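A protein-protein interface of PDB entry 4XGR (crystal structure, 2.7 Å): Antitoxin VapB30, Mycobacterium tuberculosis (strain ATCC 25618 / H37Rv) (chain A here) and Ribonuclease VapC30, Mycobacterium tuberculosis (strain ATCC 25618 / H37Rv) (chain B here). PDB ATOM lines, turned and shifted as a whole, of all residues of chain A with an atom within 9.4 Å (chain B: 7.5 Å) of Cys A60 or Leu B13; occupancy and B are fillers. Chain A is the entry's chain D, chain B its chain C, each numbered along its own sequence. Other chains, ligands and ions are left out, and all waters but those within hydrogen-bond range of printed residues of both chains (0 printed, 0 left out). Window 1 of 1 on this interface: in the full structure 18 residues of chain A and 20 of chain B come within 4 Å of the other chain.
OE2 of Glu B57 lies within salt-bridge range of NE of Arg A59.
OE2 of Glu B23 lies close to O of Leu A53 (3.3 Å).
The side-chain carboxylate (OD1) of Asp B15 lies within salt-bridge range of the guanidinium group (NH1) of Arg A57.
The backbone NH (N) of Ala A54 is in hydrogen-bond range of the side-chain carboxylate (OE2) of Glu B23 (3.4 Å).
The side-chain carboxylate (OE2) of Glu B23 lies within salt-bridge range of the guanidinium group (NE) of Arg A57, at 2.6 Å.
Of the 14 printed residues of chain A, 10 touch a printed residue of chain B.
Along chain A the printed residues that touch a printed residue of chain B span positions 53 to 65.
Among the printed residues, Asp or Glu carboxylates within 4 Å of a Lys or Arg side-chain nitrogen of the other chain: Arg A57 with Asp B15 (2.5 Å), Arg A57 with Glu B23 (2.6 Å) and Arg A59 with Glu B57 (3.4 Å).
The guanidinium group of Arg B49 sits at hydrogen-bond distance from the side-chain hydroxyl of Ser B14, at 3.2 Å.
Among the printed residues, pairs that only touch across the chains: Leu A53 with Trp B61 (3.9 Å), Ile A56 with Glu B57 (3.3 Å), Ile A56 with Trp B61 (3.6 Å), Arg A57 with Met B12 (3.1 Å), Arg A57 with Leu B13 (3.9 Å), Arg A57 with Ala B19 (3.5 Å), Cys A60 with Leu B13 (3.8 Å), Cys A60 with Phe B50 (3.9 Å), Cys A60 with Glu B57 (3.5 Å), Ala A61 with Leu B13 (3.5 Å), Ala A61 with Asp B15 (3.5 Å), Leu A63 with Phe B50 (3.6 Å), Leu A63 with Pro B53 (3.4 Å), Leu A63 with Gly B54 (3.2 Å), Pro A64 with Arg B49 (3.9 Å), Pro A64 with Phe B50 (3.5 Å), Val A65 with Arg B49 (3.5 Å) and Val A65 with Phe B50 (3.8 Å).
Cys A60 touches three residues of chain B.
Of the printed residues of chain B, Ala A61 touches Leu B13 (3.5 Å) and Asp B15 (3.5 Å).
Of the printed residues of chain A, Leu B13 touches Arg A57, Cys A60 and Ala A61.
No residue of chain A comes within 4 Å of Ser B14.
Of the printed residues of chain A, Asp B15 touches Arg A57 and Ala A61.
Of the printed residues of chain A, Pro B53 touches Leu A63 (3.4 Å).
The nearest printed residue of chain B that does not touch Ile A56 is Leu B13 (4.4 Å).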
ATOM      1  N   GLU A  52      30.345  -7.492 -13.136  1.00  0.00           N
ATOM      2  CA  GLU A  52      29.659  -7.712 -11.871  1.00  0.00           C
ATOM      3  C   GLU A  52      28.376  -8.500 -12.090  1.00  0.00           C
ATOM      4  O   GLU A  52      28.111  -9.450 -11.352  1.00  0.00           O
ATOM      5  CB  GLU A  52      29.373  -6.384 -11.170  1.00  0.00           C
ATOM      6  CG  GLU A  52      30.625  -5.578 -10.808  1.00  0.00           C
ATOM      7  CD  GLU A  52      31.058  -4.626 -11.911  1.00  0.00           C
ATOM      8  OE1 GLU A  52      31.343  -5.092 -13.044  1.00  0.00           O
ATOM      9  OE2 GLU A  52      31.097  -3.396 -11.665  1.00  0.00           O
ATOM     10  N   LEU A  53      27.616  -8.149 -13.131  1.00  0.00           N
ATOM     11  CA  LEU A  53      26.298  -8.767 -13.373  1.00  0.00           C
ATOM     12  C   LEU A  53      26.455 -10.162 -13.978  1.00  0.00           C
ATOM     13  O   LEU A  53      25.559 -10.998 -13.858  1.00  0.00           O
ATOM     14  CB  LEU A  53      25.410  -7.885 -14.261  1.00  0.00           C
ATOM     15  CG  LEU A  53      25.366  -6.381 -13.951  1.00  0.00           C
ATOM     16  CD1 LEU A  53      24.461  -5.651 -14.933  1.00  0.00           C
ATOM     17  CD2 LEU A  53      24.964  -6.122 -12.507  1.00  0.00           C
ATOM     18  N   ALA A  54      27.593 -10.397 -14.632  1.00  0.00           N
ATOM     19  CA  ALA A  54      28.046 -11.751 -14.978  1.00  0.00           C
ATOM     20  C   ALA A  54      28.503 -12.517 -13.738  1.00  0.00           C
ATOM     21  O   ALA A  54      28.135 -13.678 -13.553  1.00  0.00           O
ATOM     22  CB  ALA A  54      29.174 -11.684 -15.992  1.00  0.00           C
ATOM     23  N   ALA A  55      29.308 -11.871 -12.894  1.00  0.00           N
ATOM     24  CA  ALA A  55      29.781 -12.499 -11.653  1.00  0.00           C
ATOM     25  C   ALA A  55      28.585 -12.872 -10.792  1.00  0.00           C
ATOM     26  O   ALA A  55      28.448 -14.029 -10.398  1.00  0.00           O
ATOM     27  CB  ALA A  55      30.731 -11.583 -10.890  1.00  0.00           C
ATOM     28  N   ILE A  56      27.699 -11.901 -10.550  1.00  0.00           N
ATOM     29  CA  ILE A  56      26.437 -12.157  -9.839  1.00  0.00           C
ATOM     30  C   ILE A  56      25.623 -13.270 -10.531  1.00  0.00           C
ATOM     31  O   ILE A  56      25.179 -14.198  -9.856  1.00  0.00           O
ATOM     32  CB  ILE A  56      25.589 -10.867  -9.694  1.00  0.00           C
ATOM     33  CG1 ILE A  56      26.281  -9.876  -8.749  1.00  0.00           C
ATOM     34  CG2 ILE A  56      24.180 -11.185  -9.186  1.00  0.00           C
ATOM     35  CD1 ILE A  56      25.850  -8.443  -8.945  1.00  0.00           C
ATOM     36  N   ARG A  57      25.445 -13.181 -11.856  1.00  0.00           N
ATOM     37  CA  ARG A  57      24.683 -14.196 -12.620  1.00  0.00           C
ATOM     38  C   ARG A  57      25.291 -15.586 -12.499  1.00  0.00           C
ATOM     39  O   ARG A  57      24.589 -16.541 -12.158  1.00  0.00           O
ATOM     40  CB  ARG A  57      24.593 -13.808 -14.102  1.00  0.00           C
ATOM     41  CG  ARG A  57      24.292 -14.933 -15.087  1.00  0.00           C
ATOM     42  CD  ARG A  57      23.968 -14.339 -16.456  1.00  0.00           C
ATOM     43  NE  ARG A  57      25.125 -13.632 -17.024  1.00  0.00           N
ATOM     44  CZ  ARG A  57      26.021 -14.155 -17.875  1.00  0.00           C
ATOM     45  NH1 ARG A  57      25.925 -15.408 -18.315  1.00  0.00           N
ATOM     46  NH2 ARG A  57      27.031 -13.401 -18.298  1.00  0.00           N
ATOM     47  N   HIS A  58      26.585 -15.697 -12.804  1.00  0.00           N
ATOM     48  CA  HIS A  58      27.299 -16.968 -12.659  1.00  0.00           C
ATOM     49  C   HIS A  58      27.204 -17.439 -11.215  1.00  0.00           C
ATOM     50  O   HIS A  58      26.788 -18.567 -10.955  1.00  0.00           O
ATOM     51  CB  HIS A  58      28.774 -16.846 -13.079  1.00  0.00           C
ATOM     52  CG  HIS A  58      28.981 -16.741 -14.561  1.00  0.00           C
ATOM     53  ND1 HIS A  58      28.482 -17.671 -15.450  1.00  0.00           N
ATOM     54  CD2 HIS A  58      29.654 -15.831 -15.306  1.00  0.00           C
ATOM     55  CE1 HIS A  58      28.827 -17.330 -16.680  1.00  0.00           C
ATOM     56  NE2 HIS A  58      29.534 -16.216 -16.621  1.00  0.00           N
ATOM     57  N   ARG A  59      27.539 -16.546 -10.289  1.00  0.00           N
ATOM     58  CA  ARG A  59      27.537 -16.859  -8.858  1.00  0.00           C
ATOM     59  C   ARG A  59      26.161 -17.226  -8.336  1.00  0.00           C
ATOM     60  O   ARG A  59      26.069 -18.141  -7.525  1.00  0.00           O
ATOM     61  CB  ARG A  59      28.121 -15.705  -8.031  1.00  0.00           C
ATOM     62  CG  ARG A  59      28.321 -16.013  -6.552  1.00  0.00           C
ATOM     63  CD  ARG A  59      28.785 -14.769  -5.815  1.00  0.00           C
ATOM     64  NE  ARG A  59      29.051 -15.033  -4.402  1.00  0.00           N
ATOM     65  CZ  ARG A  59      30.166 -15.583  -3.913  1.00  0.00           C
ATOM     66  NH1 ARG A  59      31.163 -15.970  -4.715  1.00  0.00           N
ATOM     67  NH2 ARG A  59      30.282 -15.753  -2.599  1.00  0.00           N
ATOM     68  N   CYS A  60      25.117 -16.515  -8.792  1.00  0.00           N
ATOM     69  CA  CYS A  60      23.712 -16.835  -8.455  1.00  0.00           C
ATOM     70  C   CYS A  60      23.194 -18.065  -9.165  1.00  0.00           C
ATOM     71  O   CYS A  60      22.495 -18.870  -8.567  1.00  0.00           O
ATOM     72  CB  CYS A  60      22.753 -15.681  -8.778  1.00  0.00           C
ATOM     73  SG  CYS A  60      21.064 -15.913  -8.128  1.00  0.00           S
ATOM     74  N   ALA A  61      23.505 -18.191 -10.449  1.00  0.00           N
ATOM     75  CA  ALA A  61      23.079 -19.353 -11.229  1.00  0.00           C
ATOM     76  C   ALA A  61      23.620 -20.667 -10.646  1.00  0.00           C
ATOM     77  O   ALA A  61      22.910 -21.666 -10.631  1.00  0.00           O
ATOM     78  CB  ALA A  61      23.481 -19.195 -12.692  1.00  0.00           C
ATOM     79  N   ALA A  62      24.849 -20.649 -10.122  1.00  0.00           N
ATOM     80  CA  ALA A  62      25.477 -21.869  -9.566  1.00  0.00           C
ATOM     81  C   ALA A  62      24.944 -22.325  -8.194  1.00  0.00           C
ATOM     82  O   ALA A  62      25.386 -23.363  -7.693  1.00  0.00           O
ATOM     83  CB  ALA A  62      27.004 -21.713  -9.512  1.00  0.00           C
ATOM     84  N   LEU A  63      24.020 -21.572  -7.585  1.00  0.00           N
ATOM     85  CA  LEU A  63      23.314 -22.029  -6.367  1.00  0.00           C
ATOM     86  C   LEU A  63      22.537 -23.300  -6.640  1.00  0.00           C
ATOM     87  O   LEU A  63      22.108 -23.511  -7.777  1.00  0.00           O
ATOM     88  CB  LEU A  63      22.322 -20.988  -5.858  1.00  0.00           C
ATOM     89  CG  LEU A  63      22.855 -19.905  -4.928  1.00  0.00           C
ATOM     90  CD1 LEU A  63      24.159 -19.310  -5.442  1.00  0.00           C
ATOM     91  CD2 LEU A  63      21.803 -18.825  -4.746  1.00  0.00           C
ATOM     92  N   PRO A  64      22.353 -24.150  -5.608  1.00  0.00           N
ATOM     93  CA  PRO A  64      21.500 -25.322  -5.804  1.00  0.00           C
ATOM     94  C   PRO A  64      20.041 -24.929  -5.894  1.00  0.00           C
ATOM     95  O   PRO A  64      19.602 -23.997  -5.213  1.00  0.00           O
ATOM     96  CB  PRO A  64      21.765 -26.185  -4.558  1.00  0.00           C
ATOM     97  CG  PRO A  64      22.318 -25.262  -3.543  1.00  0.00           C
ATOM     98  CD  PRO A  64      23.039 -24.182  -4.300  1.00  0.00           C
ATOM     99  N   VAL A  65      19.307 -25.650  -6.736  1.00  0.00           N
ATOM    100  CA  VAL A  65      17.889 -25.404  -6.990  1.00  0.00           C
ATOM    101  C   VAL A  65      17.074 -26.073  -5.898  1.00  0.00           C
ATOM    102  O   VAL A  65      16.917 -27.290  -5.922  1.00  0.00           O
ATOM    103  CB  VAL A  65      17.465 -25.976  -8.373  1.00  0.00           C
ATOM    104  CG1 VAL A  65      15.961 -25.815  -8.600  1.00  0.00           C
ATOM    105  CG2 VAL A  65      18.238 -25.306  -9.498  1.00  0.00           C
ATOM    106  N   SER B   7      10.855 -10.815 -16.045  1.00  0.00           N
ATOM    107  CA  SER B   7      11.285 -11.868 -16.977  1.00  0.00           C
ATOM    108  C   SER B   7      12.771 -11.779 -17.303  1.00  0.00           C
ATOM    109  O   SER B   7      13.426 -12.801 -17.367  1.00  0.00           O
ATOM    110  CB  SER B   7      10.439 -11.871 -18.248  1.00  0.00           C
ATOM    111  OG  SER B   7      10.631 -10.709 -19.021  1.00  0.00           O
ATOM    112  N   ALA B   8      13.295 -10.557 -17.444  1.00  0.00           N
ATOM    113  CA  ALA B   8      14.714 -10.300 -17.784  1.00  0.00           C
ATOM    114  C   ALA B   8      15.713 -10.323 -16.608  1.00  0.00           C
ATOM    115  O   ALA B   8      16.927 -10.130 -16.834  1.00  0.00           O
ATOM    116  CB  ALA B   8      14.831  -8.961 -18.507  1.00  0.00           C
ATOM    117  N   LEU B   9      15.214 -10.491 -15.371  1.00  0.00           N
ATOM    118  CA  LEU B   9      16.067 -10.619 -14.172  1.00  0.00           C
ATOM    119  C   LEU B   9      16.055 -12.059 -13.711  1.00  0.00           C
ATOM    120  O   LEU B   9      17.096 -12.671 -13.603  1.00  0.00           O
ATOM    121  CB  LEU B   9      15.611  -9.669 -13.062  1.00  0.00           C
ATOM    122  CG  LEU B   9      16.542  -9.302 -11.883  1.00  0.00           C
ATOM    123  CD1 LEU B   9      18.006  -9.085 -12.244  1.00  0.00           C
ATOM    124  CD2 LEU B   9      16.039  -8.033 -11.209  1.00  0.00           C
ATOM    125  N   VAL B  10      14.872 -12.619 -13.503  1.00  0.00           N
ATOM    126  CA  VAL B  10      14.718 -14.063 -13.317  1.00  0.00           C
ATOM    127  C   VAL B  10      15.479 -14.813 -14.408  1.00  0.00           C
ATOM    128  O   VAL B  10      15.985 -15.906 -14.148  1.00  0.00           O
ATOM    129  CB  VAL B  10      13.223 -14.507 -13.305  1.00  0.00           C
ATOM    130  CG1 VAL B  10      13.058 -16.029 -13.372  1.00  0.00           C
ATOM    131  CG2 VAL B  10      12.530 -13.983 -12.053  1.00  0.00           C
ATOM    132  N   ALA B  11      15.538 -14.237 -15.618  1.00  0.00           N
ATOM    133  CA  ALA B  11      16.368 -14.776 -16.705  1.00  0.00           C
ATOM    134  C   ALA B  11      17.850 -14.690 -16.361  1.00  0.00           C
ATOM    135  O   ALA B  11      18.503 -15.712 -16.175  1.00  0.00           O
ATOM    136  CB  ALA B  11      16.093 -14.056 -18.019  1.00  0.00           C
ATOM    137  N   MET B  12      18.356 -13.467 -16.271  1.00  0.00           N
ATOM    138  CA  MET B  12      19.764 -13.204 -15.990  1.00  0.00           C
ATOM    139  C   MET B  12      20.254 -13.946 -14.779  1.00  0.00           C
ATOM    140  O   MET B  12      21.205 -14.705 -14.870  1.00  0.00           O
ATOM    141  CB  MET B  12      19.985 -11.712 -15.739  1.00  0.00           C
ATOM    142  CG  MET B  12      20.738 -11.046 -16.871  1.00  0.00           C
ATOM    143  SD  MET B  12      20.097  -9.197 -16.884  1.00  0.00           S
ATOM    144  CE  MET B  12      21.637  -8.018 -16.733  1.00  0.00           C
ATOM    145  N   LEU B  13      19.572 -13.828 -13.683  1.00  0.00           N
ATOM    146  CA  LEU B  13      20.028 -14.438 -12.474  1.00  0.00           C
ATOM    147  C   LEU B  13      20.028 -15.927 -12.579  1.00  0.00           C
ATOM    148  O   LEU B  13      20.709 -16.598 -11.892  1.00  0.00           O
ATOM    149  CB  LEU B  13      19.201 -13.978 -11.301  1.00  0.00           C
ATOM    150  CG  LEU B  13      19.746 -12.783 -10.529  1.00  0.00           C
ATOM    151  CD1 LEU B  13      20.451 -11.805 -11.419  1.00  0.00           C
ATOM    152  CD2 LEU B  13      18.652 -12.069  -9.774  1.00  0.00           C
ATOM    153  N   SER B  14      19.268 -16.463 -13.471  1.00  0.00           N
ATOM    154  CA  SER B  14      19.269 -17.871 -13.641  1.00  0.00           C
ATOM    155  C   SER B  14      20.142 -18.302 -14.787  1.00  0.00           C
ATOM    156  O   SER B  14      20.124 -19.422 -15.187  1.00  0.00           O
ATOM    157  CB  SER B  14      17.857 -18.355 -13.806  1.00  0.00           C
ATOM    158  OG  SER B  14      17.138 -18.125 -12.635  1.00  0.00           O
ATOM    159  N   ASP B  15      20.908 -17.385 -15.312  1.00  0.00           N
ATOM    160  CA  ASP B  15      21.770 -17.634 -16.491  1.00  0.00           C
ATOM    161  C   ASP B  15      21.014 -18.438 -17.571  1.00  0.00           C
ATOM    162  O   ASP B  15      21.399 -19.551 -17.937  1.00  0.00           O
ATOM    163  CB  ASP B  15      23.084 -18.330 -16.070  1.00  0.00           C
ATOM    164  CG  ASP B  15      24.081 -18.476 -17.220  1.00  0.00           C
ATOM    165  OD1 ASP B  15      24.739 -17.482 -17.601  1.00  0.00           O
ATOM    166  OD2 ASP B  15      24.202 -19.601 -17.733  1.00  0.00           O
ATOM    167  N   GLU B  16      19.896 -17.877 -18.018  1.00  0.00           N
ATOM    168  CA  GLU B  16      19.196 -18.370 -19.196  1.00  0.00           C
ATOM    169  C   GLU B  16      19.894 -17.785 -20.436  1.00  0.00           C
ATOM    170  O   GLU B  16      20.690 -16.841 -20.302  1.00  0.00           O
ATOM    171  CB  GLU B  16      17.714 -17.989 -19.135  1.00  0.00           C
ATOM    172  CG  GLU B  16      16.951 -18.766 -18.068  1.00  0.00           C
ATOM    173  CD  GLU B  16      15.460 -18.437 -18.024  1.00  0.00           C
ATOM    174  OE1 GLU B  16      14.974 -17.997 -16.958  1.00  0.00           O
ATOM    175  OE2 GLU B  16      14.768 -18.613 -19.052  1.00  0.00           O
ATOM    176  N   ALA B  19      21.491 -13.844 -21.683  1.00  0.00           N
ATOM    177  CA  ALA B  19      21.613 -13.031 -20.473  1.00  0.00           C
ATOM    178  C   ALA B  19      22.659 -11.916 -20.610  1.00  0.00           C
ATOM    179  O   ALA B  19      22.527 -10.861 -19.978  1.00  0.00           O
ATOM    180  CB  ALA B  19      21.949 -13.912 -19.283  1.00  0.00           C
ATOM    181  N   GLU B  23      22.570  -7.828 -20.163  1.00  0.00           N
ATOM    182  CA  GLU B  23      23.628  -7.042 -19.470  1.00  0.00           C
ATOM    183  C   GLU B  23      24.056  -5.807 -20.261  1.00  0.00           C
ATOM    184  O   GLU B  23      24.143  -4.703 -19.706  1.00  0.00           O
ATOM    185  CB  GLU B  23      24.851  -7.920 -19.112  1.00  0.00           C
ATOM    186  CG  GLU B  23      24.580  -8.983 -18.043  1.00  0.00           C
ATOM    187  CD  GLU B  23      25.742  -9.918 -17.739  1.00  0.00           C
ATOM    188  OE1 GLU B  23      26.925  -9.576 -18.005  1.00  0.00           O
ATOM    189  OE2 GLU B  23      25.451 -11.012 -17.204  1.00  0.00           O
ATOM    190  N   THR B  42       9.925 -10.792  -8.610  1.00  0.00           N
ATOM    191  CA  THR B  42      11.281 -11.242  -8.838  1.00  0.00           C
ATOM    192  C   THR B  42      11.915 -11.794  -7.562  1.00  0.00           C
ATOM    193  O   THR B  42      12.577 -12.824  -7.590  1.00  0.00           O
ATOM    194  CB  THR B  42      12.124 -10.078  -9.369  1.00  0.00           C
ATOM    195  OG1 THR B  42      11.482  -9.524 -10.524  1.00  0.00           O
ATOM    196  CG2 THR B  42      13.535 -10.536  -9.723  1.00  0.00           C
ATOM    197  N   ILE B  46      13.065 -15.796  -7.195  1.00  0.00           N
ATOM    198  CA  ILE B  46      14.437 -16.097  -6.835  1.00  0.00           C
ATOM    199  C   ILE B  46      14.506 -16.923  -5.536  1.00  0.00           C
ATOM    200  O   ILE B  46      15.070 -18.018  -5.521  1.00  0.00           O
ATOM    201  CB  ILE B  46      15.260 -14.789  -6.739  1.00  0.00           C
ATOM    202  CG1 ILE B  46      15.458 -14.184  -8.142  1.00  0.00           C
ATOM    203  CG2 ILE B  46      16.609 -15.022  -6.077  1.00  0.00           C
ATOM    204  CD1 ILE B  46      16.086 -15.112  -9.162  1.00  0.00           C
ATOM    205  N   ARG B  49      13.443 -20.458  -5.779  1.00  0.00           N
ATOM    206  CA  ARG B  49      14.324 -21.196  -6.675  1.00  0.00           C
ATOM    207  C   ARG B  49      15.614 -21.549  -5.941  1.00  0.00           C
ATOM    208  O   ARG B  49      16.010 -22.710  -5.869  1.00  0.00           O
ATOM    209  CB  ARG B  49      14.621 -20.381  -7.962  1.00  0.00           C
ATOM    210  CG  ARG B  49      15.262 -21.210  -9.081  1.00  0.00           C
ATOM    211  CD  ARG B  49      15.206 -20.561 -10.464  1.00  0.00           C
ATOM    212  NE  ARG B  49      13.849 -20.575 -11.023  1.00  0.00           N
ATOM    213  CZ  ARG B  49      13.492 -20.118 -12.230  1.00  0.00           C
ATOM    214  NH1 ARG B  49      12.211 -20.177 -12.601  1.00  0.00           N
ATOM    215  NH2 ARG B  49      14.390 -19.605 -13.070  1.00  0.00           N
ATOM    216  N   PHE B  50      16.220 -20.533  -5.352  1.00  0.00           N
ATOM    217  CA  PHE B  50      17.552 -20.620  -4.796  1.00  0.00           C
ATOM    218  C   PHE B  50      17.627 -20.316  -3.295  1.00  0.00           C
ATOM    219  O   PHE B  50      18.713 -20.171  -2.753  1.00  0.00           O
ATOM    220  CB  PHE B  50      18.442 -19.647  -5.577  1.00  0.00           C
ATOM    221  CG  PHE B  50      18.633 -20.019  -7.035  1.00  0.00           C
ATOM    222  CD1 PHE B  50      18.937 -21.336  -7.416  1.00  0.00           C
ATOM    223  CD2 PHE B  50      18.554 -19.041  -8.034  1.00  0.00           C
ATOM    224  CE1 PHE B  50      19.134 -21.663  -8.756  1.00  0.00           C
ATOM    225  CE2 PHE B  50      18.743 -19.374  -9.367  1.00  0.00           C
ATOM    226  CZ  PHE B  50      19.036 -20.686  -9.731  1.00  0.00           C
ATOM    227  N   PRO B  53      20.004 -17.397  -0.194  1.00  0.00           N
ATOM    228  CA  PRO B  53      21.207 -17.011  -0.960  1.00  0.00           C
ATOM    229  C   PRO B  53      20.912 -16.510  -2.396  1.00  0.00           C
ATOM    230  O   PRO B  53      21.681 -15.708  -2.930  1.00  0.00           O
ATOM    231  CB  PRO B  53      22.065 -18.282  -0.964  1.00  0.00           C
ATOM    232  CG  PRO B  53      21.221 -19.368  -0.394  1.00  0.00           C
ATOM    233  CD  PRO B  53      20.161 -18.720   0.434  1.00  0.00           C
ATOM    234  N   GLY B  54      19.807 -16.965  -2.992  1.00  0.00           N
ATOM    235  CA  GLY B  54      19.284 -16.354  -4.216  1.00  0.00           C
ATOM    236  C   GLY B  54      19.064 -14.872  -4.027  1.00  0.00           C
ATOM    237  O   GLY B  54      19.439 -14.061  -4.883  1.00  0.00           O
ATOM    238  N   GLY B  55      18.454 -14.525  -2.896  1.00  0.00           N
ATOM    239  CA  GLY B  55      18.120 -13.146  -2.578  1.00  0.00           C
ATOM    240  C   GLY B  55      19.284 -12.205  -2.408  1.00  0.00           C
ATOM    241  O   GLY B  55      19.179 -11.037  -2.767  1.00  0.00           O
ATOM    242  N   ARG B  56      20.377 -12.695  -1.823  1.00  0.00           N
ATOM    243  CA  ARG B  56      21.622 -11.924  -1.711  1.00  0.00           C
ATOM    244  C   ARG B  56      22.031 -11.432  -3.080  1.00  0.00           C
ATOM    245  O   ARG B  56      22.306 -10.245  -3.274  1.00  0.00           O
ATOM    246  CB  ARG B  56      22.749 -12.785  -1.116  1.00  0.00           C
ATOM    247  CG  ARG B  56      22.743 -12.863   0.407  1.00  0.00           C
ATOM    248  CD  ARG B  56      23.483 -14.085   0.952  1.00  0.00           C
ATOM    249  NE  ARG B  56      24.877 -14.189   0.498  1.00  0.00           N
ATOM    250  CZ  ARG B  56      25.668 -15.258   0.664  1.00  0.00           C
ATOM    251  NH1 ARG B  56      25.227 -16.363   1.269  1.00  0.00           N
ATOM    252  NH2 ARG B  56      26.919 -15.230   0.211  1.00  0.00           N
ATOM    253  N   GLU B  57      22.039 -12.360  -4.038  1.00  0.00           N
ATOM    254  CA  GLU B  57      22.555 -12.078  -5.379  1.00  0.00           C
ATOM    255  C   GLU B  57      21.623 -11.125  -6.108  1.00  0.00           C
ATOM    256  O   GLU B  57      22.074 -10.222  -6.834  1.00  0.00           O
ATOM    257  CB  GLU B  57      22.715 -13.374  -6.176  1.00  0.00           C
ATOM    258  CG  GLU B  57      23.687 -14.398  -5.575  1.00  0.00           C
ATOM    259  CD  GLU B  57      25.151 -13.939  -5.491  1.00  0.00           C
ATOM    260  OE1 GLU B  57      25.707 -13.316  -6.433  1.00  0.00           O
ATOM    261  OE2 GLU B  57      25.769 -14.228  -4.456  1.00  0.00           O
ATOM    262  N   LEU B  58      20.320 -11.352  -5.916  1.00  0.00           N
ATOM    263  CA  LEU B  58      19.293 -10.435  -6.371  1.00  0.00           C
ATOM    264  C   LEU B  58      19.532  -9.057  -5.808  1.00  0.00           C
ATOM    265  O   LEU B  58      19.487  -8.077  -6.554  1.00  0.00           O
ATOM    266  CB  LEU B  58      17.904 -10.927  -5.968  1.00  0.00           C
ATOM    267  CG  LEU B  58      16.680 -10.057  -6.296  1.00  0.00           C
ATOM    268  CD1 LEU B  58      16.599  -9.704  -7.772  1.00  0.00           C
ATOM    269  CD2 LEU B  58      15.426 -10.796  -5.888  1.00  0.00           C
ATOM    270  N   ASP B  59      19.790  -8.974  -4.504  1.00  0.00           N
ATOM    271  CA  ASP B  59      20.009  -7.680  -3.845  1.00  0.00           C
ATOM    272  C   ASP B  59      21.271  -6.983  -4.348  1.00  0.00           C
ATOM    273  O   ASP B  59      21.293  -5.753  -4.483  1.00  0.00           O
ATOM    274  CB  ASP B  59      20.053  -7.826  -2.312  1.00  0.00           C
ATOM    275  CG  ASP B  59      18.657  -7.966  -1.678  1.00  0.00           C
ATOM    276  OD1 ASP B  59      17.748  -7.168  -2.035  1.00  0.00           O
ATOM    277  OD2 ASP B  59      18.477  -8.865  -0.812  1.00  0.00           O
ATOM    278  N   TRP B  61      22.738  -7.418  -7.388  1.00  0.00           N
ATOM    279  CA  TRP B  61      22.405  -6.982  -8.751  1.00  0.00           C
ATOM    280  C   TRP B  61      21.713  -5.611  -8.749  1.00  0.00           C
ATOM    281  O   TRP B  61      22.115  -4.701  -9.491  1.00  0.00           O
ATOM    282  CB  TRP B  61      21.518  -8.035  -9.424  1.00  0.00           C
ATOM    283  CG  TRP B  61      21.424  -7.950 -10.907  1.00  0.00           C
ATOM    284  CD1 TRP B  61      22.033  -8.767 -11.804  1.00  0.00           C
ATOM    285  CD2 TRP B  61      20.637  -7.023 -11.676  1.00  0.00           C
ATOM    286  NE1 TRP B  61      21.702  -8.399 -13.084  1.00  0.00           N
ATOM    287  CE2 TRP B  61      20.845  -7.331 -13.036  1.00  0.00           C
ATOM    288  CE3 TRP B  61      19.776  -5.965 -11.348  1.00  0.00           C
ATOM    289  CZ2 TRP B  61      20.224  -6.622 -14.065  1.00  0.00           C
ATOM    290  CZ3 TRP B  61      19.172  -5.249 -12.373  1.00  0.00           C
ATOM    291  CH2 TRP B  61      19.397  -5.581 -13.715  1.00  0.00           C
ATOM    292  N   LEU B  62      20.684  -5.464  -7.910  1.00  0.00           N
ATOM    293  CA  LEU B  62      19.882  -4.231  -7.876  1.00  0.00           C
ATOM    294  C   LEU B  62      20.666  -3.012  -7.370  1.00  0.00           C
ATOM    295  O   LEU B  62      20.542  -1.922  -7.930  1.00  0.00           O
ATOM    296  CB  LEU B  62      18.619  -4.436  -7.031  1.00  0.00           C
ATOM    297  CG  LEU B  62      17.585  -5.431  -7.570  1.00  0.00           C
ATOM    298  CD1 LEU B  62      16.596  -5.821  -6.485  1.00  0.00           C
ATOM    299  CD2 LEU B  62      16.858  -4.860  -8.775  1.00  0.00           C
